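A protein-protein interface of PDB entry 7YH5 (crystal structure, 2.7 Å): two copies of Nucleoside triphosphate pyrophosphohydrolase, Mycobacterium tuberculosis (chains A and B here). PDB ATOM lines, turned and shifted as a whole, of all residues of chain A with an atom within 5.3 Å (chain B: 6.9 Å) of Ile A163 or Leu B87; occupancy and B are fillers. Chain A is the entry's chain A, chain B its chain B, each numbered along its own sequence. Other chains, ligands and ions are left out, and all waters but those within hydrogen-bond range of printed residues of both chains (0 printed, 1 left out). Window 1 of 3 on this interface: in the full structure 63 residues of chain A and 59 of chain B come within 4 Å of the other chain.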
ATOM      1  N   LEU A  87     -20.841 -25.014 -12.155  1.00  0.00           N
ATOM      2  CA  LEU A  87     -20.450 -23.612 -12.034  1.00  0.00           C
ATOM      3  C   LEU A  87     -19.122 -23.472 -11.300  1.00  0.00           C
ATOM      4  O   LEU A  87     -18.321 -22.586 -11.623  1.00  0.00           O
ATOM      5  CB  LEU A  87     -21.538 -22.810 -11.319  1.00  0.00           C
ATOM      6  CG  LEU A  87     -22.769 -22.373 -12.117  1.00  0.00           C
ATOM      7  CD1 LEU A  87     -23.783 -21.700 -11.203  1.00  0.00           C
ATOM      8  CD2 LEU A  87     -22.380 -21.448 -13.257  1.00  0.00           C
ATOM      9  N   VAL A  91     -15.762 -21.505 -12.450  1.00  0.00           N
ATOM     10  CA  VAL A  91     -15.002 -20.537 -11.664  1.00  0.00           C
ATOM     11  C   VAL A  91     -13.527 -20.912 -11.646  1.00  0.00           C
ATOM     12  O   VAL A  91     -12.648 -20.052 -11.794  1.00  0.00           O
ATOM     13  CB  VAL A  91     -15.582 -20.432 -10.242  1.00  0.00           C
ATOM     14  CG1 VAL A  91     -14.610 -19.708  -9.320  1.00  0.00           C
ATOM     15  CG2 VAL A  91     -16.927 -19.725 -10.274  1.00  0.00           C
ATOM     16  N   VAL A 146     -19.795 -12.181 -15.672  1.00  0.00           N
ATOM     17  CA  VAL A 146     -19.989 -12.102 -14.225  1.00  0.00           C
ATOM     18  C   VAL A 146     -18.822 -12.756 -13.493  1.00  0.00           C
ATOM     19  O   VAL A 146     -18.290 -12.205 -12.523  1.00  0.00           O
ATOM     20  CB  VAL A 146     -21.332 -12.745 -13.832  1.00  0.00           C
ATOM     21  CG1 VAL A 146     -21.491 -12.776 -12.319  1.00  0.00           C
ATOM     22  CG2 VAL A 146     -22.486 -12.002 -14.488  1.00  0.00           C
ATOM     23  N   LEU A 147     -18.408 -13.940 -13.948  1.00  0.00           N
ATOM     24  CA  LEU A 147     -17.252 -14.598 -13.344  1.00  0.00           C
ATOM     25  C   LEU A 147     -15.978 -13.797 -13.575  1.00  0.00           C
ATOM     26  O   LEU A 147     -15.137 -13.680 -12.674  1.00  0.00           O
ATOM     27  CB  LEU A 147     -17.101 -16.013 -13.903  1.00  0.00           C
ATOM     28  CG  LEU A 147     -18.329 -16.923 -13.814  1.00  0.00           C
ATOM     29  CD1 LEU A 147     -18.002 -18.318 -14.313  1.00  0.00           C
ATOM     30  CD2 LEU A 147     -18.854 -16.978 -12.392  1.00  0.00           C
ATOM     31  N   ALA A 150     -16.027 -10.743 -11.299  1.00  0.00           N
ATOM     32  CA  ALA A 150     -15.829 -11.179  -9.921  1.00  0.00           C
ATOM     33  C   ALA A 150     -14.388 -11.611  -9.682  1.00  0.00           C
ATOM     34  O   ALA A 150     -13.814 -11.332  -8.623  1.00  0.00           O
ATOM     35  CB  ALA A 150     -16.796 -12.312  -9.582  1.00  0.00           C
ATOM     36  N   GLU A 154     -11.149 -10.021  -7.131  1.00  0.00           N
ATOM     37  CA  GLU A 154     -10.289 -10.713  -6.174  1.00  0.00           C
ATOM     38  C   GLU A 154      -8.886 -10.123  -6.146  1.00  0.00           C
ATOM     39  O   GLU A 154      -8.237 -10.112  -5.093  1.00  0.00           O
ATOM     40  CB  GLU A 154     -10.222 -12.203  -6.501  1.00  0.00           C
ATOM     41  CG  GLU A 154     -11.561 -12.911  -6.496  1.00  0.00           C
ATOM     42  CD  GLU A 154     -11.414 -14.417  -6.533  1.00  0.00           C
ATOM     43  OE1 GLU A 154     -10.340 -14.917  -6.137  1.00  0.00           O
ATOM     44  OE2 GLU A 154     -12.368 -15.101  -6.960  1.00  0.00           O
ATOM     45  N   PHE A 161     -13.433  -8.663  -3.476  1.00  0.00           N
ATOM     46  CA  PHE A 161     -14.424  -9.699  -3.225  1.00  0.00           C
ATOM     47  C   PHE A 161     -14.273 -10.762  -4.307  1.00  0.00           C
ATOM     48  O   PHE A 161     -13.472 -10.621  -5.236  1.00  0.00           O
ATOM     49  CB  PHE A 161     -15.853  -9.133  -3.162  1.00  0.00           C
ATOM     50  CG  PHE A 161     -16.292  -8.394  -4.400  1.00  0.00           C
ATOM     51  CD1 PHE A 161     -16.763  -9.079  -5.509  1.00  0.00           C
ATOM     52  CD2 PHE A 161     -16.270  -7.009  -4.436  1.00  0.00           C
ATOM     53  CE1 PHE A 161     -17.180  -8.398  -6.640  1.00  0.00           C
ATOM     54  CE2 PHE A 161     -16.685  -6.322  -5.563  1.00  0.00           C
ATOM     55  CZ  PHE A 161     -17.140  -7.017  -6.666  1.00  0.00           C
ATOM     56  N   THR A 162     -15.056 -11.831  -4.186  1.00  0.00           N
ATOM     57  CA  THR A 162     -14.981 -12.974  -5.087  1.00  0.00           C
ATOM     58  C   THR A 162     -16.379 -13.318  -5.583  1.00  0.00           C
ATOM     59  O   THR A 162     -17.367 -12.665  -5.232  1.00  0.00           O
ATOM     60  CB  THR A 162     -14.361 -14.201  -4.398  1.00  0.00           C
ATOM     61  OG1 THR A 162     -15.388 -14.926  -3.708  1.00  0.00           O
ATOM     62  CG2 THR A 162     -13.283 -13.795  -3.402  1.00  0.00           C
ATOM     63  N   ILE A 163     -16.453 -14.355  -6.423  1.00  0.00           N
ATOM     64  CA  ILE A 163     -17.740 -14.817  -6.936  1.00  0.00           C
ATOM     65  C   ILE A 163     -18.634 -15.297  -5.799  1.00  0.00           C
ATOM     66  O   ILE A 163     -19.865 -15.211  -5.885  1.00  0.00           O
ATOM     67  CB  ILE A 163     -17.543 -15.904  -8.015  1.00  0.00           C
ATOM     68  CG1 ILE A 163     -18.860 -16.190  -8.741  1.00  0.00           C
ATOM     69  CG2 ILE A 163     -16.963 -17.179  -7.418  1.00  0.00           C
ATOM     70  CD1 ILE A 163     -19.442 -14.993  -9.459  1.00  0.00           C
ATOM     71  N   ASP A 164     -18.041 -15.846  -4.738  1.00  0.00           N
ATOM     72  CA  ASP A 164     -18.833 -16.263  -3.586  1.00  0.00           C
ATOM     73  C   ASP A 164     -19.501 -15.076  -2.903  1.00  0.00           C
ATOM     74  O   ASP A 164     -20.634 -15.186  -2.421  1.00  0.00           O
ATOM     75  CB  ASP A 164     -17.955 -17.031  -2.600  1.00  0.00           C
ATOM     76  CG  ASP A 164     -17.703 -18.454  -3.041  1.00  0.00           C
ATOM     77  OD1 ASP A 164     -18.688 -19.158  -3.349  1.00  0.00           O
ATOM     78  OD2 ASP A 164     -16.526 -18.865  -3.092  1.00  0.00           O
ATOM     79  N   ASP A 165     -18.816 -13.930  -2.853  1.00  0.00           N
ATOM     80  CA  ASP A 165     -19.400 -12.743  -2.232  1.00  0.00           C
ATOM     81  C   ASP A 165     -20.601 -12.225  -3.016  1.00  0.00           C
ATOM     82  O   ASP A 165     -21.638 -11.896  -2.429  1.00  0.00           O
ATOM     83  CB  ASP A 165     -18.340 -11.652  -2.089  1.00  0.00           C
ATOM     84  CG  ASP A 165     -17.336 -11.959  -0.999  1.00  0.00           C
ATOM     85  OD1 ASP A 165     -17.762 -12.257   0.137  1.00  0.00           O
ATOM     86  OD2 ASP A 165     -16.121 -11.898  -1.278  1.00  0.00           O
ATOM     87  N   VAL A 166     -20.482 -12.130  -4.342  1.00  0.00           N
ATOM     88  CA  VAL A 166     -21.619 -11.681  -5.145  1.00  0.00           C
ATOM     89  C   VAL A 166     -22.763 -12.686  -5.056  1.00  0.00           C
ATOM     90  O   VAL A 166     -23.943 -12.310  -5.077  1.00  0.00           O
ATOM     91  CB  VAL A 166     -21.184 -11.390  -6.597  1.00  0.00           C
ATOM     92  CG1 VAL A 166     -20.364 -12.511  -7.146  1.00  0.00           C
ATOM     93  CG2 VAL A 166     -22.380 -11.160  -7.476  1.00  0.00           C
ATOM     94  N   ALA A 167     -22.434 -13.976  -4.944  1.00  0.00           N
ATOM     95  CA  ALA A 167     -23.467 -14.983  -4.715  1.00  0.00           C
ATOM     96  C   ALA A 167     -24.164 -14.743  -3.382  1.00  0.00           C
ATOM     97  O   ALA A 167     -25.385 -14.917  -3.269  1.00  0.00           O
ATOM     98  CB  ALA A 167     -22.862 -16.386  -4.759  1.00  0.00           C
ATOM     99  N   ASP A 168     -23.400 -14.352  -2.358  1.00  0.00           N
ATOM    100  CA  ASP A 168     -23.988 -14.044  -1.059  1.00  0.00           C
ATOM    101  C   ASP A 168     -24.898 -12.827  -1.149  1.00  0.00           C
ATOM    102  O   ASP A 168     -25.967 -12.791  -0.529  1.00  0.00           O
ATOM    103  CB  ASP A 168     -22.887 -13.799  -0.025  1.00  0.00           C
ATOM    104  CG  ASP A 168     -22.457 -15.063   0.692  1.00  0.00           C
ATOM    105  OD1 ASP A 168     -23.217 -16.055   0.668  1.00  0.00           O
ATOM    106  OD2 ASP A 168     -21.360 -15.062   1.289  1.00  0.00           O
ATOM    107  N   ARG B   9     -21.991 -28.731   3.118  1.00  0.00           N
ATOM    108  CA  ARG B   9     -22.779 -29.103   1.952  1.00  0.00           C
ATOM    109  C   ARG B   9     -22.785 -30.604   1.706  1.00  0.00           C
ATOM    110  O   ARG B   9     -23.591 -31.084   0.903  1.00  0.00           O
ATOM    111  CB  ARG B   9     -22.268 -28.360   0.714  1.00  0.00           C
ATOM    112  CG  ARG B   9     -22.670 -26.891   0.723  1.00  0.00           C
ATOM    113  CD  ARG B   9     -22.230 -26.123  -0.510  1.00  0.00           C
ATOM    114  NE  ARG B   9     -22.433 -24.688  -0.317  1.00  0.00           N
ATOM    115  CZ  ARG B   9     -21.565 -23.882   0.291  1.00  0.00           C
ATOM    116  NH1 ARG B   9     -20.424 -24.367   0.762  1.00  0.00           N
ATOM    117  NH2 ARG B   9     -21.836 -22.592   0.431  1.00  0.00           N
ATOM    118  N   ARG B  83     -13.921 -22.293  -4.197  1.00  0.00           N
ATOM    119  CA  ARG B  83     -14.427 -21.037  -4.741  1.00  0.00           C
ATOM    120  C   ARG B  83     -15.621 -21.282  -5.654  1.00  0.00           C
ATOM    121  O   ARG B  83     -15.527 -22.037  -6.627  1.00  0.00           O
ATOM    122  CB  ARG B  83     -13.302 -20.335  -5.505  1.00  0.00           C
ATOM    123  CG  ARG B  83     -13.551 -18.884  -5.896  1.00  0.00           C
ATOM    124  CD  ARG B  83     -13.942 -18.004  -4.717  1.00  0.00           C
ATOM    125  NE  ARG B  83     -13.062 -18.152  -3.559  1.00  0.00           N
ATOM    126  CZ  ARG B  83     -11.831 -17.655  -3.472  1.00  0.00           C
ATOM    127  NH1 ARG B  83     -11.305 -16.976  -4.482  1.00  0.00           N
ATOM    128  NH2 ARG B  83     -11.122 -17.841  -2.367  1.00  0.00           N
ATOM    129  N   GLY B  84     -16.747 -20.653  -5.329  1.00  0.00           N
ATOM    130  CA  GLY B  84     -17.943 -20.744  -6.139  1.00  0.00           C
ATOM    131  C   GLY B  84     -19.000 -21.718  -5.668  1.00  0.00           C
ATOM    132  O   GLY B  84     -19.921 -22.016  -6.437  1.00  0.00           O
ATOM    133  N   GLU B  85     -18.909 -22.224  -4.437  1.00  0.00           N
ATOM    134  CA  GLU B  85     -19.896 -23.198  -3.982  1.00  0.00           C
ATOM    135  C   GLU B  85     -21.169 -22.527  -3.483  1.00  0.00           C
ATOM    136  O   GLU B  85     -22.237 -23.149  -3.497  1.00  0.00           O
ATOM    137  CB  GLU B  85     -19.295 -24.095  -2.900  1.00  0.00           C
ATOM    138  CG  GLU B  85     -18.279 -25.085  -3.456  1.00  0.00           C
ATOM    139  CD  GLU B  85     -18.160 -26.353  -2.635  1.00  0.00           C
ATOM    140  OE1 GLU B  85     -17.053 -26.629  -2.124  1.00  0.00           O
ATOM    141  OE2 GLU B  85     -19.170 -27.075  -2.504  1.00  0.00           O
ATOM    142  N   ARG B  86     -21.079 -21.268  -3.047  1.00  0.00           N
ATOM    143  CA  ARG B  86     -22.290 -20.512  -2.756  1.00  0.00           C
ATOM    144  C   ARG B  86     -23.127 -20.315  -4.012  1.00  0.00           C
ATOM    145  O   ARG B  86     -24.347 -20.146  -3.923  1.00  0.00           O
ATOM    146  CB  ARG B  86     -21.934 -19.165  -2.124  1.00  0.00           C
ATOM    147  N   LEU B  87     -22.490 -20.335  -5.188  1.00  0.00           N
ATOM    148  CA  LEU B  87     -23.235 -20.328  -6.444  1.00  0.00           C
ATOM    149  C   LEU B  87     -24.198 -21.504  -6.517  1.00  0.00           C
ATOM    150  O   LEU B  87     -25.329 -21.363  -6.995  1.00  0.00           O
ATOM    151  CB  LEU B  87     -22.271 -20.367  -7.632  1.00  0.00           C
ATOM    152  CG  LEU B  87     -21.640 -19.064  -8.122  1.00  0.00           C
ATOM    153  CD1 LEU B  87     -20.535 -19.359  -9.127  1.00  0.00           C
ATOM    154  CD2 LEU B  87     -22.695 -18.165  -8.733  1.00  0.00           C
ATOM    155  N   VAL B  88     -23.764 -22.678  -6.053  1.00  0.00           N
ATOM    156  CA  VAL B  88     -24.657 -23.831  -6.011  1.00  0.00           C
ATOM    157  C   VAL B  88     -25.785 -23.591  -5.015  1.00  0.00           C
ATOM    158  O   VAL B  88     -26.929 -24.005  -5.243  1.00  0.00           O
ATOM    159  CB  VAL B  88     -23.859 -25.107  -5.685  1.00  0.00           C
ATOM    160  CG1 VAL B  88     -24.782 -26.314  -5.590  1.00  0.00           C
ATOM    161  CG2 VAL B  88     -22.782 -25.335  -6.735  1.00  0.00           C
ATOM    162  N   ASP B  89     -25.490 -22.912  -3.901  1.00  0.00           N
ATOM    163  CA  ASP B  89     -26.565 -22.456  -3.024  1.00  0.00           C
ATOM    164  C   ASP B  89     -27.504 -21.512  -3.760  1.00  0.00           C
ATOM    165  O   ASP B  89     -28.711 -21.502  -3.493  1.00  0.00           O
ATOM    166  CB  ASP B  89     -26.001 -21.757  -1.782  1.00  0.00           C
ATOM    167  CG  ASP B  89     -24.987 -22.601  -1.032  1.00  0.00           C
ATOM    168  OD1 ASP B  89     -24.052 -22.017  -0.442  1.00  0.00           O
ATOM    169  OD2 ASP B  89     -25.127 -23.841  -1.022  1.00  0.00           O
ATOM    170  N   ALA B  90     -26.972 -20.729  -4.704  1.00  0.00           N
ATOM    171  CA  ALA B  90     -27.775 -19.714  -5.377  1.00  0.00           C
ATOM    172  C   ALA B  90     -28.765 -20.336  -6.355  1.00  0.00           C
ATOM    173  O   ALA B  90     -29.929 -19.920  -6.409  1.00  0.00           O
ATOM    174  CB  ALA B  90     -26.865 -18.716  -6.094  1.00  0.00           C
ATOM    175  N   VAL B  91     -28.333 -21.327  -7.137  1.00  0.00           N
ATOM    176  CA  VAL B  91     -29.252 -21.916  -8.105  1.00  0.00           C
ATOM    177  C   VAL B  91     -30.355 -22.694  -7.398  1.00  0.00           C
ATOM    178  O   VAL B  91     -31.444 -22.883  -7.953  1.00  0.00           O
ATOM    179  CB  VAL B  91     -28.497 -22.806  -9.105  1.00  0.00           C
ATOM    180  CG1 VAL B  91     -27.214 -22.132  -9.553  1.00  0.00           C
ATOM    181  CG2 VAL B  91     -28.217 -24.153  -8.498  1.00  0.00           C
ATOM    182  N   ALA B  92     -30.103 -23.154  -6.169  1.00  0.00           N
ATOM    183  CA  ALA B  92     -31.148 -23.836  -5.414  1.00  0.00           C
ATOM    184  C   ALA B  92     -32.227 -22.855  -4.981  1.00  0.00           C
ATOM    185  O   ALA B  92     -33.423 -23.165  -5.052  1.00  0.00           O
ATOM    186  CB  ALA B  92     -30.547 -24.550  -4.204  1.00  0.00           C
ATOM    187  N   LEU B 139     -23.497  -6.785 -10.040  1.00  0.00           N
ATOM    188  CA  LEU B 139     -22.980  -8.062 -10.518  1.00  0.00           C
ATOM    189  C   LEU B 139     -23.896  -9.205 -10.105  1.00  0.00           C
ATOM    190  O   LEU B 139     -24.130 -10.136 -10.884  1.00  0.00           O
ATOM    191  CB  LEU B 139     -21.563  -8.290  -9.989  1.00  0.00           C
ATOM    192  CG  LEU B 139     -20.434  -8.172 -11.011  1.00  0.00           C
ATOM    193  CD1 LEU B 139     -19.095  -8.476 -10.358  1.00  0.00           C
ATOM    194  CD2 LEU B 139     -20.686  -9.096 -12.189  1.00  0.00           C
ATOM    195  N   LEU B 143     -26.107 -11.911 -12.442  1.00  0.00           N
ATOM    196  CA  LEU B 143     -26.099 -13.344 -12.183  1.00  0.00           C
ATOM    197  C   LEU B 143     -27.512 -13.866 -11.939  1.00  0.00           C
ATOM    198  O   LEU B 143     -27.830 -15.000 -12.306  1.00  0.00           O
ATOM    199  CB  LEU B 143     -25.185 -13.648 -10.997  1.00  0.00           C
ATOM    200  CG  LEU B 143     -25.340 -14.973 -10.249  1.00  0.00           C
ATOM    201  CD1 LEU B 143     -24.780 -16.141 -11.055  1.00  0.00           C
ATOM    202  CD2 LEU B 143     -24.673 -14.882  -8.881  1.00  0.00           C
ATOM    203  N   LEU B 147     -29.340 -17.078 -13.866  1.00  0.00           N
ATOM    204  CA  LEU B 147     -29.924 -18.242 -13.198  1.00  0.00           C
ATOM    205  C   LEU B 147     -31.429 -18.360 -13.443  1.00  0.00           C
ATOM    206  O   LEU B 147     -31.973 -19.472 -13.430  1.00  0.00           O
ATOM    207  CB  LEU B 147     -29.654 -18.185 -11.692  1.00  0.00           C
ATOM    208  CG  LEU B 147     -28.189 -18.003 -11.299  1.00  0.00           C
ATOM    209  CD1 LEU B 147     -28.058 -17.865  -9.798  1.00  0.00           C
ATOM    210  CD2 LEU B 147     -27.322 -19.149 -11.803  1.00  0.00           C
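OE1 of Glu A154 lies within salt-bridge range of NH1 of Arg B83 (2.8 Å).
The side-chain carboxylate (OD2) of Asp A164 lies within salt-bridge range of the guanidinium group (NE) of Arg B83 (3.6 Å).
The backbone NH (N) of Gly B84 lies within hydrogen-bond range of the side-chain carboxylate (OD2) of Asp A164.
OD1 of Asp A164 sits at hydrogen-bond distance from N of Glu B85 (3.3 Å).
The backbone NH (N) of Arg B86 sits at hydrogen-bond distance from the side-chain carboxylate (OD1) of Asp A164.
The backbone NH (N) of Glu A154 is in hydrogen-bond range of the backbone carbonyl oxygen (O) of Phe A161, at 3.1 Å.
The side-chain hydroxyl (OG1) of Thr A162 sits at hydrogen-bond distance from the backbone NH (N) of Asp A164 (3.0 Å).
N of Thr A162 sits at hydrogen-bond distance from OD2 of Asp A165.
Among the printed residues, merely in contact across the chains: Leu A87 with Val B91 (3.8 Å), Val A91 with Arg B83 (3.7 Å), Val A91 with Leu B87 (3.8 Å), Val A146 with Leu B139 (3.7 Å), Ala A150 with Leu B139 (3.9 Å), Thr A162 with Arg B83 (3.5 Å), Ile A163 with Gly B84 (3.9 Å), Ile A163 with Leu B87 (3.6 Å), Val A166 with Leu B139 (3.6 Å), Ala A167 with Arg B86 (3.9 Å) and Ala A167 with Leu B87 (3.99 Å).
Of the printed residues of chain B, Val A91 touches Arg B83 (3.7 Å) and Leu B87 (3.8 Å).
Printed residues of chain B within 4 Å of Thr A162: Arg B83 (3.5 Å).
Ile A163 touches two residues of chain B.
Of the printed residues of chain A, Gly B84 touches Ile A163 and Asp A164.
Printed residues of chain A within 4 Å of Arg B86: Asp A164 and Ala A167.
Printed residues of chain A within 4 Å of Leu B87: Val A91, Ile A163 and Ala A167.
Leu B143 touches none of the printed residues of chain A.
The nearest residue of chain B that does not touch Ile A163 is Arg B83 (4.1 Å).
The nearest printed residue of chain A that does not touch Leu B87 is Leu A87 (4.1 Å).
Of the 14 printed residues of chain B, 7 touch a printed residue of chain A.
Hydrophobic or aromatic side chains of chain B within 4 Å of the printed part of chain A: Leu B87, Val B91 and Leu B139.
Along chain B the printed residues that touch a printed residue of chain A span positions 83 to 139.
Leu A87 touches Val B91, and with the chains exchanged Val A91 touches Leu B87.
Of the 16 pairs that touch across the chains among the printed residues, 2 have their exchanged pair printed and touching as well.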
